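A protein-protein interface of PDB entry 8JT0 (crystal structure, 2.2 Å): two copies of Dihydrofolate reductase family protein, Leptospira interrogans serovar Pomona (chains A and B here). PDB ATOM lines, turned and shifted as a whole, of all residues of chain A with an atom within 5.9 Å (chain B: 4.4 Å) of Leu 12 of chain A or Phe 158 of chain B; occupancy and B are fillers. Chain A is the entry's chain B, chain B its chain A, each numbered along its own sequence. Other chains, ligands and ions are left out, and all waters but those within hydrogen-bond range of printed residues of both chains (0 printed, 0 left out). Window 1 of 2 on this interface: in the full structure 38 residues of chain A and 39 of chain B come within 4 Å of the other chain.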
ATOM      1  N   ILE A  10      22.644  14.631 -15.997  1.00  0.00           N
ATOM      2  CA  ILE A  10      23.594  13.724 -15.358  1.00  0.00           C
ATOM      3  C   ILE A  10      23.196  13.458 -13.918  1.00  0.00           C
ATOM      4  O   ILE A  10      22.561  14.286 -13.259  1.00  0.00           O
ATOM      5  CB  ILE A  10      25.051  14.240 -15.416  1.00  0.00           C
ATOM      6  CG1 ILE A  10      25.208  15.543 -14.614  1.00  0.00           C
ATOM      7  CG2 ILE A  10      25.510  14.396 -16.861  1.00  0.00           C
ATOM      8  CD1 ILE A  10      26.515  16.222 -14.855  1.00  0.00           C
ATOM      9  N   THR A  11      23.565  12.269 -13.442  1.00  0.00           N
ATOM     10  CA  THR A  11      23.466  11.930 -12.032  1.00  0.00           C
ATOM     11  C   THR A  11      24.564  12.643 -11.241  1.00  0.00           C
ATOM     12  O   THR A  11      25.434  13.316 -11.795  1.00  0.00           O
ATOM     13  CB  THR A  11      23.587  10.425 -11.830  1.00  0.00           C
ATOM     14  OG1 THR A  11      24.867   9.994 -12.328  1.00  0.00           O
ATOM     15  CG2 THR A  11      22.479   9.706 -12.593  1.00  0.00           C
ATOM     16  N   LEU A  12      24.526  12.473  -9.924  1.00  0.00           N
ATOM     17  CA  LEU A  12      25.581  13.019  -9.082  1.00  0.00           C
ATOM     18  C   LEU A  12      26.950  12.476  -9.490  1.00  0.00           C
ATOM     19  O   LEU A  12      27.941  13.217  -9.502  1.00  0.00           O
ATOM     20  CB  LEU A  12      25.272  12.703  -7.620  1.00  0.00           C
ATOM     21  CG  LEU A  12      24.489  13.777  -6.868  1.00  0.00           C
ATOM     22  CD1 LEU A  12      24.488  13.472  -5.378  1.00  0.00           C
ATOM     23  CD2 LEU A  12      25.099  15.135  -7.129  1.00  0.00           C
ATOM     24  N   ASP A  13      27.026  11.201  -9.881  1.00  0.00           N
ATOM     25  CA  ASP A  13      28.310  10.630 -10.260  1.00  0.00           C
ATOM     26  C   ASP A  13      28.567  10.687 -11.759  1.00  0.00           C
ATOM     27  O   ASP A  13      29.440   9.969 -12.254  1.00  0.00           O
ATOM     28  CB  ASP A  13      28.450   9.196  -9.742  1.00  0.00           C
ATOM     29  CG  ASP A  13      27.340   8.273 -10.202  1.00  0.00           C
ATOM     30  OD1 ASP A  13      26.149   8.671 -10.180  1.00  0.00           O
ATOM     31  OD2 ASP A  13      27.669   7.116 -10.546  1.00  0.00           O
ATOM     32  N   GLY A  14      27.835  11.525 -12.488  1.00  0.00           N
ATOM     33  CA  GLY A  14      28.162  11.736 -13.910  1.00  0.00           C
ATOM     34  C   GLY A  14      27.524  10.798 -14.915  1.00  0.00           C
ATOM     35  O   GLY A  14      27.967  10.824 -16.066  1.00  0.00           O
ATOM     36  N   VAL A  15      26.524  10.012 -14.534  1.00  0.00           N
ATOM     37  CA  VAL A  15      25.968   9.047 -15.528  1.00  0.00           C
ATOM     38  C   VAL A  15      24.892   9.760 -16.356  1.00  0.00           C
ATOM     39  O   VAL A  15      24.071  10.467 -15.762  1.00  0.00           O
ATOM     40  CB  VAL A  15      25.472   7.754 -14.859  1.00  0.00           C
ATOM     41  CG1 VAL A  15      24.620   6.912 -15.794  1.00  0.00           C
ATOM     42  CG2 VAL A  15      26.633   6.938 -14.317  1.00  0.00           C
ATOM     43  N   ILE A 146      21.780  18.394 -12.845  1.00  0.00           N
ATOM     44  CA  ILE A 146      22.384  17.418 -11.951  1.00  0.00           C
ATOM     45  C   ILE A 146      21.317  16.928 -10.990  1.00  0.00           C
ATOM     46  O   ILE A 146      20.711  17.721 -10.258  1.00  0.00           O
ATOM     47  CB  ILE A 146      23.591  18.011 -11.208  1.00  0.00           C
ATOM     48  CG1 ILE A 146      24.624  18.488 -12.229  1.00  0.00           C
ATOM     49  CG2 ILE A 146      24.222  16.964 -10.298  1.00  0.00           C
ATOM     50  CD1 ILE A 146      25.700  19.376 -11.666  1.00  0.00           C
ATOM     51  N   PHE A 147      21.101  15.619 -10.985  1.00  0.00           N
ATOM     52  CA  PHE A 147      19.975  14.978 -10.336  1.00  0.00           C
ATOM     53  C   PHE A 147      20.401  14.254  -9.058  1.00  0.00           C
ATOM     54  O   PHE A 147      21.447  13.597  -9.031  1.00  0.00           O
ATOM     55  CB  PHE A 147      19.300  13.988 -11.309  1.00  0.00           C
ATOM     56  CG  PHE A 147      18.560  14.665 -12.458  1.00  0.00           C
ATOM     57  CD1 PHE A 147      19.252  15.200 -13.537  1.00  0.00           C
ATOM     58  CD2 PHE A 147      17.177  14.772 -12.444  1.00  0.00           C
ATOM     59  CE1 PHE A 147      18.573  15.827 -14.577  1.00  0.00           C
ATOM     60  CE2 PHE A 147      16.493  15.405 -13.480  1.00  0.00           C
ATOM     61  CZ  PHE A 147      17.185  15.926 -14.542  1.00  0.00           C
ATOM     62  N   PRO A 148      19.612  14.338  -8.000  1.00  0.00           N
ATOM     63  CA  PRO A 148      20.034  13.877  -6.672  1.00  0.00           C
ATOM     64  C   PRO A 148      20.030  12.362  -6.497  1.00  0.00           C
ATOM     65  O   PRO A 148      19.472  11.829  -5.532  1.00  0.00           O
ATOM     66  CB  PRO A 148      19.012  14.540  -5.746  1.00  0.00           C
ATOM     67  CG  PRO A 148      17.787  14.642  -6.576  1.00  0.00           C
ATOM     68  CD  PRO A 148      18.263  14.931  -7.981  1.00  0.00           C
ATOM     69  N   VAL A 149      20.674  11.688  -7.450  1.00  0.00           N
ATOM     70  CA  VAL A 149      20.733  10.202  -7.423  1.00  0.00           C
ATOM     71  C   VAL A 149      22.140   9.742  -7.795  1.00  0.00           C
ATOM     72  O   VAL A 149      22.872  10.514  -8.422  1.00  0.00           O
ATOM     73  CB  VAL A 149      19.722   9.567  -8.398  1.00  0.00           C
ATOM     74  CG1 VAL A 149      18.289   9.713  -7.925  1.00  0.00           C
ATOM     75  CG2 VAL A 149      19.883  10.093  -9.814  1.00  0.00           C
ATOM     76  N   THR A 150      22.482   8.525  -7.398  1.00  0.00           N
ATOM     77  CA  THR A 150      23.774   7.945  -7.819  1.00  0.00           C
ATOM     78  C   THR A 150      23.490   6.575  -8.435  1.00  0.00           C
ATOM     79  O   THR A 150      22.599   5.891  -7.929  1.00  0.00           O
ATOM     80  CB  THR A 150      24.779   7.948  -6.664  1.00  0.00           C
ATOM     81  OG1 THR A 150      26.023   7.533  -7.220  1.00  0.00           O
ATOM     82  CG2 THR A 150      24.380   7.064  -5.507  1.00  0.00           C
ATOM     83  N   ASN A 152      26.091   3.600 -10.077  1.00  0.00           N
ATOM     84  CA  ASN A 152      27.499   3.350 -10.486  1.00  0.00           C
ATOM     85  C   ASN A 152      27.599   3.115 -11.993  1.00  0.00           C
ATOM     86  O   ASN A 152      28.384   3.820 -12.640  1.00  0.00           O
ATOM     87  CB  ASN A 152      28.107   2.163  -9.749  1.00  0.00           C
ATOM     88  CG  ASN A 152      29.555   2.390  -9.371  1.00  0.00           C
ATOM     89  OD1 ASN A 152      30.174   3.354  -9.813  1.00  0.00           O
ATOM     90  ND2 ASN A 152      30.103   1.513  -8.546  1.00  0.00           N
ATOM     91  N   GLN B 131      34.896   4.745  -0.254  1.00  0.00           N
ATOM     92  CA  GLN B 131      34.357   3.653  -1.068  1.00  0.00           C
ATOM     93  C   GLN B 131      33.696   2.582  -0.198  1.00  0.00           C
ATOM     94  O   GLN B 131      32.589   2.109  -0.513  1.00  0.00           O
ATOM     95  CB  GLN B 131      35.445   3.032  -1.949  1.00  0.00           C
ATOM     96  CG  GLN B 131      36.038   3.995  -2.964  1.00  0.00           C
ATOM     97  CD  GLN B 131      34.983   4.904  -3.554  1.00  0.00           C
ATOM     98  OE1 GLN B 131      34.031   4.446  -4.208  1.00  0.00           O
ATOM     99  NE2 GLN B 131      35.118   6.203  -3.294  1.00  0.00           N
ATOM    100  N   PHE B 134      30.361   3.965   1.178  1.00  0.00           N
ATOM    101  CA  PHE B 134      29.321   3.959   0.147  1.00  0.00           C
ATOM    102  C   PHE B 134      28.767   2.559  -0.058  1.00  0.00           C
ATOM    103  O   PHE B 134      27.549   2.354  -0.035  1.00  0.00           O
ATOM    104  CB  PHE B 134      29.883   4.489  -1.177  1.00  0.00           C
ATOM    105  CG  PHE B 134      29.929   5.988  -1.266  1.00  0.00           C
ATOM    106  CD1 PHE B 134      29.164   6.771  -0.420  1.00  0.00           C
ATOM    107  CD2 PHE B 134      30.746   6.610  -2.193  1.00  0.00           C
ATOM    108  CE1 PHE B 134      29.207   8.155  -0.502  1.00  0.00           C
ATOM    109  CE2 PHE B 134      30.794   7.994  -2.279  1.00  0.00           C
ATOM    110  CZ  PHE B 134      30.026   8.765  -1.432  1.00  0.00           C
ATOM    111  N   LEU B 142      25.886  14.174   2.484  1.00  0.00           N
ATOM    112  CA  LEU B 142      26.937  14.495   1.526  1.00  0.00           C
ATOM    113  C   LEU B 142      26.995  15.998   1.349  1.00  0.00           C
ATOM    114  O   LEU B 142      26.063  16.588   0.794  1.00  0.00           O
ATOM    115  CB  LEU B 142      26.676  13.856   0.161  1.00  0.00           C
ATOM    116  CG  LEU B 142      27.095  12.448  -0.216  1.00  0.00           C
ATOM    117  CD1 LEU B 142      27.597  12.498  -1.663  1.00  0.00           C
ATOM    118  CD2 LEU B 142      28.166  11.961   0.698  1.00  0.00           C
ATOM    119  N   ARG B 156      38.674   9.539  -7.444  1.00  0.00           N
ATOM    120  CA  ARG B 156      37.327  10.160  -7.488  1.00  0.00           C
ATOM    121  C   ARG B 156      36.494   9.776  -6.263  1.00  0.00           C
ATOM    122  O   ARG B 156      36.766   8.727  -5.676  1.00  0.00           O
ATOM    123  CB  ARG B 156      36.659   9.794  -8.814  1.00  0.00           C
ATOM    124  CG  ARG B 156      36.395   8.313  -9.029  1.00  0.00           C
ATOM    125  CD  ARG B 156      35.766   8.139 -10.398  1.00  0.00           C
ATOM    126  NE  ARG B 156      36.172   9.198 -11.310  1.00  0.00           N
ATOM    127  CZ  ARG B 156      35.341  10.032 -11.923  1.00  0.00           C
ATOM    128  NH1 ARG B 156      34.039   9.937 -11.727  1.00  0.00           N
ATOM    129  NH2 ARG B 156      35.820  10.965 -12.725  1.00  0.00           N
ATOM    130  N   LEU B 157      35.526  10.621  -5.902  1.00  0.00           N
ATOM    131  CA  LEU B 157      34.637  10.354  -4.743  1.00  0.00           C
ATOM    132  C   LEU B 157      33.742   9.165  -5.075  1.00  0.00           C
ATOM    133  O   LEU B 157      33.651   8.245  -4.260  1.00  0.00           O
ATOM    134  CB  LEU B 157      33.793  11.601  -4.485  1.00  0.00           C
ATOM    135  CG  LEU B 157      32.673  11.448  -3.462  1.00  0.00           C
ATOM    136  CD1 LEU B 157      33.240  11.147  -2.089  1.00  0.00           C
ATOM    137  CD2 LEU B 157      31.828  12.705  -3.419  1.00  0.00           C
ATOM    138  N   PHE B 158      33.117   9.206  -6.243  1.00  0.00           N
ATOM    139  CA  PHE B 158      32.204   8.114  -6.648  1.00  0.00           C
ATOM    140  C   PHE B 158      33.023   7.075  -7.412  1.00  0.00           C
ATOM    141  O   PHE B 158      33.084   7.138  -8.642  1.00  0.00           O
ATOM    142  CB  PHE B 158      31.017   8.698  -7.412  1.00  0.00           C
ATOM    143  CG  PHE B 158      30.207   9.705  -6.642  1.00  0.00           C
ATOM    144  CD1 PHE B 158      29.510   9.334  -5.507  1.00  0.00           C
ATOM    145  CD2 PHE B 158      30.137  11.024  -7.055  1.00  0.00           C
ATOM    146  CE1 PHE B 158      28.760  10.261  -4.803  1.00  0.00           C
ATOM    147  CE2 PHE B 158      29.383  11.948  -6.352  1.00  0.00           C
ATOM    148  CZ  PHE B 158      28.696  11.565  -5.228  1.00  0.00           C
ATOM    149  N   GLY B 159      33.613   6.137  -6.676  1.00  0.00           N
ATOM    150  CA  GLY B 159      34.464   5.123  -7.309  1.00  0.00           C
ATOM    151  C   GLY B 159      33.907   3.720  -7.215  1.00  0.00           C
ATOM    152  O   GLY B 159      32.693   3.571  -7.368  1.00  0.00           O
ATOM    153  N   THR B 162      30.657   3.058  -5.029  1.00  0.00           N
ATOM    154  CA  THR B 162      29.381   3.747  -5.339  1.00  0.00           C
ATOM    155  C   THR B 162      28.278   2.723  -5.626  1.00  0.00           C
ATOM    156  O   THR B 162      28.547   1.750  -6.343  1.00  0.00           O
ATOM    157  CB  THR B 162      29.555   4.720  -6.508  1.00  0.00           C
ATOM    158  OG1 THR B 162      30.909   5.161  -6.491  1.00  0.00           O
ATOM    159  CG2 THR B 162      28.616   5.901  -6.431  1.00  0.00           C
ATOM    160  N   TYR B 184      23.297  17.189   0.447  1.00  0.00           N
ATOM    161  CA  TYR B 184      22.292  16.157   0.208  1.00  0.00           C
ATOM    162  C   TYR B 184      22.138  15.231   1.410  1.00  0.00           C
ATOM    163  O   TYR B 184      23.090  14.996   2.165  1.00  0.00           O
ATOM    164  CB  TYR B 184      22.656  15.274  -0.994  1.00  0.00           C
ATOM    165  CG  TYR B 184      22.809  15.985  -2.308  1.00  0.00           C
ATOM    166  CD1 TYR B 184      21.754  16.052  -3.212  1.00  0.00           C
ATOM    167  CD2 TYR B 184      24.014  16.572  -2.662  1.00  0.00           C
ATOM    168  CE1 TYR B 184      21.898  16.696  -4.433  1.00  0.00           C
ATOM    169  CE2 TYR B 184      24.165  17.215  -3.876  1.00  0.00           C
ATOM    170  CZ  TYR B 184      23.098  17.278  -4.761  1.00  0.00           C
ATOM    171  OH  TYR B 184      23.256  17.921  -5.974  1.00  0.00           O
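The backbone carbonyl oxygen (O) of Thr 162 of chain B sits at hydrogen-bond distance from the side-chain amide nitrogen (ND2) of Asn 152 of chain A, at 2.7 Å.
The side-chain carboxylate of Asp 13 of chain A is in hydrogen-bond range of the side-chain hydroxyl of Thr 11 of chain A (2.8 Å).
OD1 of Asp 13 of chain A sits at hydrogen-bond distance from OG1 of Thr 150 of chain A (3.2 Å).
The backbone NH (N) of Leu 12 of chain A lies within hydrogen-bond range of the backbone carbonyl oxygen (O) of Val 149 of chain A (3.0 Å).
The side-chain hydroxyl (OG1) of Thr 162 of chain B sits at hydrogen-bond distance from the backbone carbonyl oxygen (O) of Gly 159 of chain B (2.5 Å).
N of Leu 12 of chain A is in hydrogen-bond range of O of Phe 147 of chain A (3.4 Å).
O of Leu 142 of chain B is in hydrogen-bond range of N of Tyr 184 of chain B (2.9 Å).
Leu 12 of chain A touches Phe 158 of chain B.
Tyr 184 of chain B touches Leu 12 of chain A (OH to CD2, 3.5 Å).
Asp 13 of chain A touches Phe 158 of chain B.
CE1 of Tyr 184 of chain B touches CB of Pro 148 of chain A (3.8 Å).
Thr 150 of chain A touches Thr 162 of chain B (OG1 to CG2, 3.2 Å).
Asn 152 of chain A touches Gly 159 of chain B (ND2 to O, 3.5 Å).
Of chain B, only Phe 158 (3.7 Å) and Tyr 184 (3.5 Å) come within 4 Å of Leu 12 of chain A.
Of chain A, only Leu 12 (3.7 Å) and Asp 13 (3.5 Å) come within 4 Å of Phe 158 of chain B.
Printed residues of chain B within 4 Å of Asp 13 of chain A: Phe 158.
Of the printed residues of chain B, Thr 150 of chain A touches Thr 162 (3.2 Å).
Of the printed residues of chain B, Pro 148 of chain A touches Tyr 184 (3.8 Å).
Val 149 of chain A touches none of the printed residues of chain B.
The nearest printed residue of chain B that does not touch Leu 12 of chain A is Leu 142 of chain B (4.9 Å).
Of the 12 printed residues of chain A, 5 touch a printed residue of chain B.
Printed residues of chain A that touch a printed residue of chain B: Leu 12, Asp 13, Pro 148, Thr 150 and Asn 152.
Hydrophobic or aromatic side chains of chain A within 4 Å of the printed part of chain B: Leu 12 and Pro 148.
Along chain A the printed residues that touch a printed residue of chain B span positions 12 to 152.
Of the 9 printed residues of chain B, 4 touch a printed residue of chain A.
Among the printed residues, 7 pairs touch across the chains.
Among the printed residues, no Asp or Glu carboxylate lies within 4 Å of a Lys or Arg side-chain nitrogen of the other chain.
No position is printed for both chains.
Of the 7 pairs that touch across the chains among the printed residues, none has its exchanged pair printed and touching as well.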
